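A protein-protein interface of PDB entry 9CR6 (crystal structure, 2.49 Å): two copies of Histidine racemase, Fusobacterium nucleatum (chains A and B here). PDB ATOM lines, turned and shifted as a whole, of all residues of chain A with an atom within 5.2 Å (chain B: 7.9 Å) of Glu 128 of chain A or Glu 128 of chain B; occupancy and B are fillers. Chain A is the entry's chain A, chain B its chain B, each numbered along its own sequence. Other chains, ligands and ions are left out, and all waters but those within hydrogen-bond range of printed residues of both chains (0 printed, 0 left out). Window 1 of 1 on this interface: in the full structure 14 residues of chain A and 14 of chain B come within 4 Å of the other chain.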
ATOM      1  N   SER A 126      27.045 -35.181   2.484  1.00  0.00           N
ATOM      2  CA  SER A 126      26.190 -34.224   1.792  1.00  0.00           C
ATOM      3  C   SER A 126      25.668 -34.869   0.518  1.00  0.00           C
ATOM      4  O   SER A 126      26.369 -35.653  -0.124  1.00  0.00           O
ATOM      5  CB  SER A 126      26.950 -32.933   1.467  1.00  0.00           C
ATOM      6  OG  SER A 126      28.103 -33.202   0.690  1.00  0.00           O
ATOM      7  N   LEU A 127      24.429 -34.527   0.160  1.00  0.00           N
ATOM      8  CA  LEU A 127      23.757 -35.056  -1.023  1.00  0.00           C
ATOM      9  C   LEU A 127      23.391 -33.895  -1.934  1.00  0.00           C
ATOM     10  O   LEU A 127      22.860 -32.882  -1.467  1.00  0.00           O
ATOM     11  CB  LEU A 127      22.511 -35.852  -0.619  1.00  0.00           C
ATOM     12  CG  LEU A 127      21.405 -36.085  -1.646  1.00  0.00           C
ATOM     13  CD1 LEU A 127      21.890 -36.949  -2.801  1.00  0.00           C
ATOM     14  CD2 LEU A 127      20.202 -36.735  -0.966  1.00  0.00           C
ATOM     15  N   GLU A 128      23.671 -34.040  -3.230  1.00  0.00           N
ATOM     16  CA  GLU A 128      23.522 -32.940  -4.170  1.00  0.00           C
ATOM     17  C   GLU A 128      22.926 -33.438  -5.479  1.00  0.00           C
ATOM     18  O   GLU A 128      22.668 -34.634  -5.659  1.00  0.00           O
ATOM     19  CB  GLU A 128      24.870 -32.256  -4.438  1.00  0.00           C
ATOM     20  CG  GLU A 128      25.876 -32.396  -3.312  1.00  0.00           C
ATOM     21  CD  GLU A 128      27.171 -31.678  -3.617  1.00  0.00           C
ATOM     22  OE1 GLU A 128      27.406 -31.353  -4.802  1.00  0.00           O
ATOM     23  OE2 GLU A 128      27.949 -31.431  -2.672  1.00  0.00           O
ATOM     24  N   GLU A 129      22.714 -32.496  -6.405  1.00  0.00           N
ATOM     25  CA  GLU A 129      22.181 -32.796  -7.736  1.00  0.00           C
ATOM     26  C   GLU A 129      22.809 -31.793  -8.709  1.00  0.00           C
ATOM     27  O   GLU A 129      22.303 -30.684  -8.887  1.00  0.00           O
ATOM     28  CB  GLU A 129      20.663 -32.725  -7.758  1.00  0.00           C
ATOM     29  CG  GLU A 129      19.972 -34.055  -7.486  1.00  0.00           C
ATOM     30  CD  GLU A 129      18.936 -33.964  -6.380  1.00  0.00           C
ATOM     31  OE1 GLU A 129      18.330 -32.884  -6.213  1.00  0.00           O
ATOM     32  OE2 GLU A 129      18.727 -34.976  -5.678  1.00  0.00           O
ATOM     33  N   ILE A 130      23.913 -32.198  -9.330  1.00  0.00           N
ATOM     34  CA  ILE A 130      24.622 -31.332 -10.262  1.00  0.00           C
ATOM     35  C   ILE A 130      23.902 -31.318 -11.604  1.00  0.00           C
ATOM     36  O   ILE A 130      23.209 -32.271 -11.976  1.00  0.00           O
ATOM     37  CB  ILE A 130      26.092 -31.776 -10.416  1.00  0.00           C
ATOM     38  CG1 ILE A 130      26.182 -33.224 -10.895  1.00  0.00           C
ATOM     39  CG2 ILE A 130      26.830 -31.613  -9.097  1.00  0.00           C
ATOM     40  CD1 ILE A 130      27.521 -33.885 -10.613  1.00  0.00           C
ATOM     41  N   ASN A 131      24.060 -30.213 -12.335  1.00  0.00           N
ATOM     42  CA  ASN A 131      23.447 -30.009 -13.644  1.00  0.00           C
ATOM     43  C   ASN A 131      24.494 -29.599 -14.672  1.00  0.00           C
ATOM     44  O   ASN A 131      24.240 -28.775 -15.554  1.00  0.00           O
ATOM     45  CB  ASN A 131      22.337 -28.962 -13.576  1.00  0.00           C
ATOM     46  CG  ASN A 131      21.140 -29.432 -12.777  1.00  0.00           C
ATOM     47  OD1 ASN A 131      20.123 -29.835 -13.341  1.00  0.00           O
ATOM     48  ND2 ASN A 131      21.253 -29.378 -11.452  1.00  0.00           N
ATOM     49  N   LEU A 137      23.159 -35.237 -12.674  1.00  0.00           N
ATOM     50  CA  LEU A 137      23.774 -36.317 -11.922  1.00  0.00           C
ATOM     51  C   LEU A 137      23.539 -36.113 -10.434  1.00  0.00           C
ATOM     52  O   LEU A 137      23.613 -34.990  -9.932  1.00  0.00           O
ATOM     53  CB  LEU A 137      25.282 -36.385 -12.186  1.00  0.00           C
ATOM     54  CG  LEU A 137      25.753 -37.161 -13.416  1.00  0.00           C
ATOM     55  CD1 LEU A 137      25.722 -36.273 -14.649  1.00  0.00           C
ATOM     56  CD2 LEU A 137      27.153 -37.709 -13.186  1.00  0.00           C
ATOM     57  N   GLY A 138      23.252 -37.205  -9.730  1.00  0.00           N
ATOM     58  CA  GLY A 138      23.289 -37.171  -8.287  1.00  0.00           C
ATOM     59  C   GLY A 138      24.710 -37.327  -7.781  1.00  0.00           C
ATOM     60  O   GLY A 138      25.574 -37.887  -8.452  1.00  0.00           O
ATOM     61  N   LEU A 139      24.961 -36.806  -6.582  1.00  0.00           N
ATOM     62  CA  LEU A 139      26.283 -36.925  -5.976  1.00  0.00           C
ATOM     63  C   LEU A 139      26.111 -37.045  -4.470  1.00  0.00           C
ATOM     64  O   LEU A 139      25.713 -36.082  -3.810  1.00  0.00           O
ATOM     65  CB  LEU A 139      27.169 -35.734  -6.335  1.00  0.00           C
ATOM     66  CG  LEU A 139      28.446 -35.559  -5.506  1.00  0.00           C
ATOM     67  CD1 LEU A 139      29.212 -36.863  -5.347  1.00  0.00           C
ATOM     68  CD2 LEU A 139      29.347 -34.504  -6.132  1.00  0.00           C
ATOM     69  N   VAL A 140      26.404 -38.225  -3.937  1.00  0.00           N
ATOM     70  CA  VAL A 140      26.490 -38.449  -2.500  1.00  0.00           C
ATOM     71  C   VAL A 140      27.968 -38.522  -2.143  1.00  0.00           C
ATOM     72  O   VAL A 140      28.716 -39.322  -2.723  1.00  0.00           O
ATOM     73  CB  VAL A 140      25.752 -39.730  -2.080  1.00  0.00           C
ATOM     74  CG1 VAL A 140      25.482 -39.714  -0.583  1.00  0.00           C
ATOM     75  CG2 VAL A 140      24.453 -39.880  -2.863  1.00  0.00           C
ATOM     76  N   ARG A 141      28.394 -37.686  -1.201  1.00  0.00           N
ATOM     77  CA  ARG A 141      29.793 -37.583  -0.808  1.00  0.00           C
ATOM     78  C   ARG A 141      29.971 -38.224   0.559  1.00  0.00           C
ATOM     79  O   ARG A 141      29.333 -37.807   1.532  1.00  0.00           O
ATOM     80  CB  ARG A 141      30.251 -36.122  -0.777  1.00  0.00           C
ATOM     81  CG  ARG A 141      29.436 -35.187  -1.658  1.00  0.00           C
ATOM     82  CD  ARG A 141      29.996 -33.770  -1.637  1.00  0.00           C
ATOM     83  NE  ARG A 141      31.248 -33.665  -2.380  1.00  0.00           N
ATOM     84  CZ  ARG A 141      31.414 -32.965  -3.496  1.00  0.00           C
ATOM     85  NH1 ARG A 141      30.421 -32.284  -4.045  1.00  0.00           N
ATOM     86  NH2 ARG A 141      32.610 -32.952  -4.078  1.00  0.00           N
ATOM     87  N   TYR A 170      34.776 -32.577 -13.584  1.00  0.00           N
ATOM     88  CA  TYR A 170      34.166 -31.936 -12.423  1.00  0.00           C
ATOM     89  C   TYR A 170      35.114 -31.932 -11.230  1.00  0.00           C
ATOM     90  O   TYR A 170      35.166 -30.955 -10.474  1.00  0.00           O
ATOM     91  CB  TYR A 170      32.859 -32.653 -12.075  1.00  0.00           C
ATOM     92  CG  TYR A 170      32.107 -32.075 -10.897  1.00  0.00           C
ATOM     93  CD1 TYR A 170      32.508 -32.336  -9.593  1.00  0.00           C
ATOM     94  CD2 TYR A 170      30.983 -31.283 -11.088  1.00  0.00           C
ATOM     95  CE1 TYR A 170      31.820 -31.816  -8.515  1.00  0.00           C
ATOM     96  CE2 TYR A 170      30.288 -30.757 -10.017  1.00  0.00           C
ATOM     97  CZ  TYR A 170      30.711 -31.029  -8.731  1.00  0.00           C
ATOM     98  OH  TYR A 170      30.028 -30.514  -7.654  1.00  0.00           O
ATOM     99  N   PHE B 124      28.222 -20.173 -16.448  1.00  0.00           N
ATOM    100  CA  PHE B 124      28.499 -21.104 -15.363  1.00  0.00           C
ATOM    101  C   PHE B 124      28.974 -22.447 -15.906  1.00  0.00           C
ATOM    102  O   PHE B 124      28.556 -22.895 -16.978  1.00  0.00           O
ATOM    103  CB  PHE B 124      27.248 -21.306 -14.500  1.00  0.00           C
ATOM    104  CG  PHE B 124      26.194 -22.172 -15.138  1.00  0.00           C
ATOM    105  CD1 PHE B 124      25.729 -21.907 -16.415  1.00  0.00           C
ATOM    106  CD2 PHE B 124      25.663 -23.251 -14.452  1.00  0.00           C
ATOM    107  CE1 PHE B 124      24.758 -22.705 -16.998  1.00  0.00           C
ATOM    108  CE2 PHE B 124      24.692 -24.053 -15.031  1.00  0.00           C
ATOM    109  CZ  PHE B 124      24.239 -23.775 -16.303  1.00  0.00           C
ATOM    110  N   LEU B 125      29.865 -23.089 -15.149  1.00  0.00           N
ATOM    111  CA  LEU B 125      30.328 -24.422 -15.519  1.00  0.00           C
ATOM    112  C   LEU B 125      29.317 -25.489 -15.114  1.00  0.00           C
ATOM    113  O   LEU B 125      29.060 -26.424 -15.880  1.00  0.00           O
ATOM    114  CB  LEU B 125      31.687 -24.707 -14.876  1.00  0.00           C
ATOM    115  CG  LEU B 125      32.739 -23.604 -15.000  1.00  0.00           C
ATOM    116  CD1 LEU B 125      33.890 -23.845 -14.034  1.00  0.00           C
ATOM    117  CD2 LEU B 125      33.248 -23.509 -16.431  1.00  0.00           C
ATOM    118  N   SER B 126      28.734 -25.359 -13.924  1.00  0.00           N
ATOM    119  CA  SER B 126      27.757 -26.316 -13.429  1.00  0.00           C
ATOM    120  C   SER B 126      26.830 -25.614 -12.449  1.00  0.00           C
ATOM    121  O   SER B 126      27.130 -24.527 -11.949  1.00  0.00           O
ATOM    122  CB  SER B 126      28.434 -27.518 -12.757  1.00  0.00           C
ATOM    123  OG  SER B 126      29.510 -27.099 -11.937  1.00  0.00           O
ATOM    124  N   LEU B 127      25.695 -26.256 -12.174  1.00  0.00           N
ATOM    125  CA  LEU B 127      24.685 -25.721 -11.268  1.00  0.00           C
ATOM    126  C   LEU B 127      24.197 -26.851 -10.376  1.00  0.00           C
ATOM    127  O   LEU B 127      23.659 -27.842 -10.873  1.00  0.00           O
ATOM    128  CB  LEU B 127      23.521 -25.101 -12.048  1.00  0.00           C
ATOM    129  CG  LEU B 127      22.291 -24.676 -11.244  1.00  0.00           C
ATOM    130  CD1 LEU B 127      22.666 -23.667 -10.171  1.00  0.00           C
ATOM    131  CD2 LEU B 127      21.234 -24.098 -12.172  1.00  0.00           C
ATOM    132  N   GLU B 128      24.367 -26.693  -9.066  1.00  0.00           N
ATOM    133  CA  GLU B 128      24.120 -27.758  -8.110  1.00  0.00           C
ATOM    134  C   GLU B 128      23.095 -27.332  -7.065  1.00  0.00           C
ATOM    135  O   GLU B 128      22.710 -26.167  -6.966  1.00  0.00           O
ATOM    136  CB  GLU B 128      25.424 -28.176  -7.415  1.00  0.00           C
ATOM    137  CG  GLU B 128      26.614 -28.284  -8.346  1.00  0.00           C
ATOM    138  CD  GLU B 128      27.854 -28.793  -7.639  1.00  0.00           C
ATOM    139  OE1 GLU B 128      27.723 -29.667  -6.753  1.00  0.00           O
ATOM    140  OE2 GLU B 128      28.962 -28.326  -7.971  1.00  0.00           O
ATOM    141  N   GLU B 129      22.658 -28.321  -6.276  1.00  0.00           N
ATOM    142  CA  GLU B 129      21.726 -28.126  -5.160  1.00  0.00           C
ATOM    143  C   GLU B 129      22.207 -29.047  -4.037  1.00  0.00           C
ATOM    144  O   GLU B 129      21.723 -30.171  -3.899  1.00  0.00           O
ATOM    145  CB  GLU B 129      20.291 -28.430  -5.573  1.00  0.00           C
ATOM    146  CG  GLU B 129      19.294 -28.502  -4.416  1.00  0.00           C
ATOM    147  CD  GLU B 129      18.196 -29.540  -4.637  1.00  0.00           C
ATOM    148  OE1 GLU B 129      18.220 -30.235  -5.678  1.00  0.00           O
ATOM    149  OE2 GLU B 129      17.309 -29.661  -3.765  1.00  0.00           O
ATOM    150  N   ILE B 130      23.153 -28.562  -3.239  1.00  0.00           N
ATOM    151  CA  ILE B 130      23.781 -29.391  -2.220  1.00  0.00           C
ATOM    152  C   ILE B 130      22.910 -29.420  -0.972  1.00  0.00           C
ATOM    153  O   ILE B 130      22.232 -28.444  -0.634  1.00  0.00           O
ATOM    154  CB  ILE B 130      25.205 -28.890  -1.907  1.00  0.00           C
ATOM    155  CG1 ILE B 130      25.186 -27.812  -0.825  1.00  0.00           C
ATOM    156  CG2 ILE B 130      25.873 -28.340  -3.164  1.00  0.00           C
ATOM    157  CD1 ILE B 130      26.564 -27.256  -0.490  1.00  0.00           C
ATOM    158  N   ASN B 131      22.934 -30.554  -0.273  1.00  0.00           N
ATOM    159  CA  ASN B 131      22.189 -30.751   0.971  1.00  0.00           C
ATOM    160  C   ASN B 131      23.192 -31.132   2.057  1.00  0.00           C
ATOM    161  O   ASN B 131      23.353 -32.311   2.383  1.00  0.00           O
ATOM    162  CB  ASN B 131      21.099 -31.831   0.808  1.00  0.00           C
ATOM    163  CG  ASN B 131      20.042 -31.449  -0.209  1.00  0.00           C
ATOM    164  OD1 ASN B 131      19.029 -30.834   0.129  1.00  0.00           O
ATOM    165  ND2 ASN B 131      20.268 -31.821  -1.463  1.00  0.00           N
ATOM    166  N   VAL B 132      23.877 -30.130   2.610  1.00  0.00           N
ATOM    167  CA  VAL B 132      24.796 -30.344   3.719  1.00  0.00           C
ATOM    168  C   VAL B 132      24.055 -30.080   5.021  1.00  0.00           C
ATOM    169  O   VAL B 132      23.177 -29.213   5.097  1.00  0.00           O
ATOM    170  CB  VAL B 132      26.046 -29.448   3.610  1.00  0.00           C
ATOM    171  CG1 VAL B 132      27.194 -30.042   4.417  1.00  0.00           C
ATOM    172  CG2 VAL B 132      26.452 -29.260   2.159  1.00  0.00           C
ATOM    173  N   LEU B 137      21.356 -25.729  -0.168  1.00  0.00           N
ATOM    174  CA  LEU B 137      22.119 -24.608  -0.688  1.00  0.00           C
ATOM    175  C   LEU B 137      22.281 -24.740  -2.192  1.00  0.00           C
ATOM    176  O   LEU B 137      22.449 -25.845  -2.714  1.00  0.00           O
ATOM    177  CB  LEU B 137      23.504 -24.526  -0.035  1.00  0.00           C
ATOM    178  CG  LEU B 137      23.573 -23.990   1.395  1.00  0.00           C
ATOM    179  CD1 LEU B 137      23.465 -25.128   2.394  1.00  0.00           C
ATOM    180  CD2 LEU B 137      24.864 -23.211   1.598  1.00  0.00           C
ATOM    181  N   GLY B 138      22.233 -23.604  -2.887  1.00  0.00           N
ATOM    182  CA  GLY B 138      22.557 -23.579  -4.292  1.00  0.00           C
ATOM    183  C   GLY B 138      24.045 -23.418  -4.522  1.00  0.00           C
ATOM    184  O   GLY B 138      24.787 -23.009  -3.631  1.00  0.00           O
ATOM    185  N   LEU B 139      24.481 -23.757  -5.732  1.00  0.00           N
ATOM    186  CA  LEU B 139      25.878 -23.601  -6.114  1.00  0.00           C
ATOM    187  C   LEU B 139      25.950 -23.418  -7.621  1.00  0.00           C
ATOM    188  O   LEU B 139      25.375 -24.209  -8.372  1.00  0.00           O
ATOM    189  CB  LEU B 139      26.718 -24.807  -5.680  1.00  0.00           C
ATOM    190  CG  LEU B 139      28.183 -24.504  -5.355  1.00  0.00           C
ATOM    191  CD1 LEU B 139      28.877 -25.733  -4.785  1.00  0.00           C
ATOM    192  CD2 LEU B 139      28.919 -24.006  -6.583  1.00  0.00           C
ATOM    193  N   VAL B 140      26.650 -22.372  -8.052  1.00  0.00           N
ATOM    194  CA  VAL B 140      26.860 -22.082  -9.471  1.00  0.00           C
ATOM    195  C   VAL B 140      28.366 -21.937  -9.657  1.00  0.00           C
ATOM    196  O   VAL B 140      28.929 -20.850  -9.492  1.00  0.00           O
ATOM    197  CB  VAL B 140      26.118 -20.825  -9.933  1.00  0.00           C
ATOM    198  CG1 VAL B 140      26.093 -20.759 -11.448  1.00  0.00           C
ATOM    199  CG2 VAL B 140      24.709 -20.804  -9.361  1.00  0.00           C
ATOM    200  N   ARG B 141      29.033 -23.036  -9.997  1.00  0.00           N
ATOM    201  CA  ARG B 141      30.482 -23.014 -10.152  1.00  0.00           C
ATOM    202  C   ARG B 141      30.869 -22.210 -11.386  1.00  0.00           C
ATOM    203  O   ARG B 141      30.330 -22.424 -12.478  1.00  0.00           O
ATOM    204  CB  ARG B 141      31.023 -24.442 -10.253  1.00  0.00           C
ATOM    205  CG  ARG B 141      30.560 -25.348  -9.123  1.00  0.00           C
ATOM    206  CD  ARG B 141      31.261 -26.694  -9.137  1.00  0.00           C
ATOM    207  NE  ARG B 141      31.061 -27.406  -7.880  1.00  0.00           N
ATOM    208  CZ  ARG B 141      32.033 -27.793  -7.060  1.00  0.00           C
ATOM    209  NH1 ARG B 141      33.306 -27.555  -7.333  1.00  0.00           N
ATOM    210  NH2 ARG B 141      31.717 -28.437  -5.941  1.00  0.00           N
ATOM    211  N   ASN B 146      33.245 -19.686  -6.822  1.00  0.00           N
ATOM    212  CA  ASN B 146      32.133 -20.571  -6.504  1.00  0.00           C
ATOM    213  C   ASN B 146      31.089 -19.756  -5.749  1.00  0.00           C
ATOM    214  O   ASN B 146      31.374 -19.226  -4.668  1.00  0.00           O
ATOM    215  CB  ASN B 146      32.594 -21.764  -5.671  1.00  0.00           C
ATOM    216  CG  ASN B 146      33.720 -22.535  -6.333  1.00  0.00           C
ATOM    217  OD1 ASN B 146      33.584 -23.013  -7.461  1.00  0.00           O
ATOM    218  ND2 ASN B 146      34.844 -22.658  -5.633  1.00  0.00           N
ATOM    219  N   HIS B 147      29.891 -19.654  -6.317  1.00  0.00           N
ATOM    220  CA  HIS B 147      28.835 -18.790  -5.796  1.00  0.00           C
ATOM    221  C   HIS B 147      27.728 -19.655  -5.206  1.00  0.00           C
ATOM    222  O   HIS B 147      26.920 -20.233  -5.940  1.00  0.00           O
ATOM    223  CB  HIS B 147      28.299 -17.879  -6.897  1.00  0.00           C
ATOM    224  CG  HIS B 147      29.046 -16.589  -7.032  1.00  0.00           C
ATOM    225  ND1 HIS B 147      29.313 -15.769  -5.958  1.00  0.00           N
ATOM    226  CD2 HIS B 147      29.587 -15.980  -8.114  1.00  0.00           C
ATOM    227  CE1 HIS B 147      29.984 -14.711  -6.371  1.00  0.00           C
ATOM    228  NE2 HIS B 147      30.164 -14.814  -7.676  1.00  0.00           N
ATOM    229  N   PHE B 148      27.689 -19.734  -3.881  1.00  0.00           N
ATOM    230  CA  PHE B 148      26.646 -20.468  -3.182  1.00  0.00           C
ATOM    231  C   PHE B 148      25.424 -19.581  -2.982  1.00  0.00           C
ATOM    232  O   PHE B 148      25.530 -18.356  -2.878  1.00  0.00           O
ATOM    233  CB  PHE B 148      27.152 -20.979  -1.830  1.00  0.00           C
ATOM    234  CG  PHE B 148      28.334 -21.902  -1.935  1.00  0.00           C
ATOM    235  CD1 PHE B 148      29.612 -21.395  -2.103  1.00  0.00           C
ATOM    236  CD2 PHE B 148      28.168 -23.277  -1.874  1.00  0.00           C
ATOM    237  CE1 PHE B 148      30.703 -22.238  -2.205  1.00  0.00           C
ATOM    238  CE2 PHE B 148      29.256 -24.128  -1.976  1.00  0.00           C
ATOM    239  CZ  PHE B 148      30.525 -23.607  -2.142  1.00  0.00           C
ATOM    240  N   ILE B 149      24.258 -20.216  -2.933  1.00  0.00           N
ATOM    241  CA  ILE B 149      22.988 -19.529  -2.739  1.00  0.00           C
ATOM    242  C   ILE B 149      22.334 -20.075  -1.479  1.00  0.00           C
ATOM    243  O   ILE B 149      22.456 -21.262  -1.156  1.00  0.00           O
ATOM    244  CB  ILE B 149      22.067 -19.696  -3.970  1.00  0.00           C
ATOM    245  CG1 ILE B 149      22.319 -18.569  -4.976  1.00  0.00           C
ATOM    246  CG2 ILE B 149      20.595 -19.709  -3.567  1.00  0.00           C
ATOM    247  CD1 ILE B 149      23.637 -18.687  -5.718  1.00  0.00           C
ATOM    248  N   TYR B 170      32.683 -27.175   3.798  1.00  0.00           N
ATOM    249  CA  TYR B 170      32.328 -27.933   2.603  1.00  0.00           C
ATOM    250  C   TYR B 170      33.441 -27.894   1.562  1.00  0.00           C
ATOM    251  O   TYR B 170      33.620 -28.861   0.814  1.00  0.00           O
ATOM    252  CB  TYR B 170      31.025 -27.387   2.014  1.00  0.00           C
ATOM    253  CG  TYR B 170      30.643 -27.981   0.677  1.00  0.00           C
ATOM    254  CD1 TYR B 170      31.155 -27.465  -0.507  1.00  0.00           C
ATOM    255  CD2 TYR B 170      29.762 -29.051   0.596  1.00  0.00           C
ATOM    256  CE1 TYR B 170      30.809 -28.001  -1.730  1.00  0.00           C
ATOM    257  CE2 TYR B 170      29.410 -29.595  -0.626  1.00  0.00           C
ATOM    258  CZ  TYR B 170      29.938 -29.065  -1.785  1.00  0.00           C
ATOM    259  OH  TYR B 170      29.595 -29.595  -3.009  1.00  0.00           O
ATOM    260  N   GLU B 174      38.615 -28.807  -1.232  1.00  0.00           N
ATOM    261  CA  GLU B 174      38.445 -28.252  -2.567  1.00  0.00           C
ATOM    262  C   GLU B 174      39.366 -27.052  -2.706  1.00  0.00           C
ATOM    263  O   GLU B 174      39.238 -26.080  -1.955  1.00  0.00           O
ATOM    264  CB  GLU B 174      36.984 -27.852  -2.800  1.00  0.00           C
ATOM    265  CG  GLU B 174      36.723 -27.206  -4.145  1.00  0.00           C
ATOM    266  CD  GLU B 174      35.452 -27.714  -4.804  1.00  0.00           C
ATOM    267  OE1 GLU B 174      34.529 -28.148  -4.083  1.00  0.00           O
ATOM    268  OE2 GLU B 174      35.378 -27.675  -6.051  1.00  0.00           O
ATOM    269  N   TYR B 219      20.362 -19.898 -10.811  1.00  0.00           N
ATOM    270  CA  TYR B 219      19.637 -20.723  -9.850  1.00  0.00           C
ATOM    271  C   TYR B 219      18.138 -20.453  -9.893  1.00  0.00           C
ATOM    272  O   TYR B 219      17.343 -21.335  -9.546  1.00  0.00           O
ATOM    273  CB  TYR B 219      20.212 -20.481  -8.451  1.00  0.00           C
ATOM    274  CG  TYR B 219      19.284 -20.793  -7.299  1.00  0.00           C
ATOM    275  CD1 TYR B 219      18.411 -19.836  -6.812  1.00  0.00           C
ATOM    276  CD2 TYR B 219      19.300 -22.039  -6.683  1.00  0.00           C
ATOM    277  CE1 TYR B 219      17.564 -20.107  -5.759  1.00  0.00           C
ATOM    278  CE2 TYR B 219      18.458 -22.319  -5.622  1.00  0.00           C
ATOM    279  CZ  TYR B 219      17.591 -21.347  -5.166  1.00  0.00           C
ATOM    280  OH  TYR B 219      16.744 -21.608  -4.112  1.00  0.00           O
ATOM    281  N   LYS B 222      16.583 -22.308 -13.130  1.00  0.00           N
ATOM    282  CA  LYS B 222      16.422 -23.747 -12.962  1.00  0.00           C
ATOM    283  C   LYS B 222      15.308 -24.073 -11.975  1.00  0.00           C
ATOM    284  O   LYS B 222      14.579 -25.054 -12.161  1.00  0.00           O
ATOM    285  CB  LYS B 222      17.742 -24.365 -12.493  1.00  0.00           C
ATOM    286  CG  LYS B 222      18.000 -25.777 -13.005  1.00  0.00           C
ATOM    287  CD  LYS B 222      17.535 -26.827 -12.008  1.00  0.00           C
ATOM    288  CE  LYS B 222      18.545 -27.025 -10.885  1.00  0.00           C
ATOM    289  NZ  LYS B 222      18.130 -28.105  -9.942  1.00  0.00           N
ATOM    290  N   CYS B 223      15.154 -23.259 -10.930  1.00  0.00           N
ATOM    291  CA  CYS B 223      14.212 -23.557  -9.859  1.00  0.00           C
ATOM    292  C   CYS B 223      12.853 -22.900 -10.052  1.00  0.00           C
ATOM    293  O   CYS B 223      11.852 -23.410  -9.534  1.00  0.00           O
ATOM    294  CB  CYS B 223      14.797 -23.115  -8.514  1.00  0.00           C
ATOM    295  SG  CYS B 223      16.044 -24.240  -7.848  1.00  0.00           S
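Of the printed residues of chain B, Ser 126 of chain A touches Asn 131 and Val 132. Glu 128 of chain A touches four residues of chain B. Of the printed residues of chain B, Ile 130 of chain A touches Leu 127 and Glu 128. Of the printed residues of chain B, Arg 141 of chain A touches Tyr 170 (3.0 Å). Printed residues of chain A within 4 Å of Leu 127 of chain B: Glu 129 (3.7 Å), Ile 130 (3.6 Å) and Asn 131 (2.8 Å). Of chain A, only Glu 128 (2.6 Å), Glu 129 (3.5 Å), Ile 130 (3.2 Å) and Tyr 170 (2.5 Å) come within 4 Å of Glu 128 of chain B. Printed residues of chain A within 4 Å of Arg 141 of chain B: Tyr 170 (3.2 Å). The nearest residue of chain A that does not touch Glu 128 of chain B is Arg 141 of chain A (4.6 Å). The nearest printed residue of chain B that does not touch Arg 141 of chain A is Arg 141 of chain B (4.5 Å).
O of Leu 127 of chain A lies within hydrogen-bond range of N of Asn 131 of chain B, 2.6 Å away. The side-chain carboxylate (OE1) of Glu 129 of chain B sits close to the side-chain carboxylate (OE1) of Glu 129 of chain A, at 2.7 Å. The backbone NH of Asn 131 of chain A sits at hydrogen-bond distance from the backbone carbonyl oxygen of Leu 127 of chain B, 2.8 Å away. The side-chain carboxylate of Glu 128 of chain A lies close to the side-chain carboxylate of Glu 128 of chain B. The guanidinium group (NH2) of Arg 141 of chain B is in hydrogen-bond range of the side-chain hydroxyl (OH) of Tyr 170 of chain A, at 3.2 Å. The side-chain carboxylate of Glu 128 of chain A is in hydrogen-bond range of the side-chain hydroxyl of Tyr 170 of chain B, 2.5 Å away. OH of Tyr 170 of chain B is in hydrogen-bond range of NH1 of Arg 141 of chain A (3.0 Å). The side-chain carboxylate (OE2) of Glu 128 of chain B lies within hydrogen-bond range of the side-chain hydroxyl (OH) of Tyr 170 of chain A (2.5 Å).
Among the printed residues, merely in contact across the chains: Ile 130 of chain A with Glu 128 of chain B (3.2 Å), Glu 128 of chain A with Glu 129 of chain B (3.3 Å), Ser 126 of chain A with Asn 131 of chain B (3.5 Å), Leu 127 of chain A with Ile 130 of chain B (3.5 Å), Glu 129 of chain A with Glu 128 of chain B (3.5 Å), Ile 130 of chain A with Leu 127 of chain B (3.6 Å), Glu 128 of chain A with Ile 130 of chain B (3.6 Å), Asn 131 of chain A with Lys 222 of chain B (3.6 Å), Glu 129 of chain A with Leu 127 of chain B (3.7 Å), Ser 126 of chain A with Val 132 of chain B (3.8 Å) and Leu 127 of chain A with Glu 129 of chain B (3.8 Å).
The backbone NH (N) of Glu 128 of chain A lies within hydrogen-bond range of the backbone carbonyl oxygen (O) of Leu 139 of chain A, 2.9 Å away. The side-chain carboxylate of Glu 128 of chain A lies within salt-bridge range of the guanidinium group of Arg 141 of chain A, 3.0 Å away. The backbone carbonyl oxygen (O) of Ser 126 of chain B sits at hydrogen-bond distance from the backbone NH (N) of Arg 141 of chain B, 3.1 Å away. OE2 of Glu 174 of chain B lies within salt-bridge range of NH1 of Arg 141 of chain B, at 2.4 Å.
Hydrophobic or aromatic side chains of chain A that line the printed part of chain B: Ile 130 and Tyr 170. Hydrophobic or aromatic side chains of chain B within 4 Å of the printed part of chain A: Ile 130, Val 132 and Tyr 170. Among the printed residues, no Asp or Glu carboxylate lies within 4 Å of a Lys or Arg side-chain nitrogen of the other chain.
Ser 126 of chain A touches Asn 131 of chain B, but with the chains exchanged Asn 131 of chain A does not touch Ser 126 of chain B (4.8 Å). Leu 127 of chain A touches Ile 130 of chain B, and with the chains exchanged Ile 130 of chain A touches Leu 127 of chain B. Leu 127 of chain A touches Asn 131 of chain B, and with the chains exchanged Asn 131 of chain A touches Leu 127 of chain B. Glu 128 of chain A touches Glu 129 of chain B, and with the chains exchanged Glu 129 of chain A touches Glu 128 of chain B. Of the 19 pairs that touch across the chains among the printed residues, 16 have their exchanged pair printed and touching as well.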
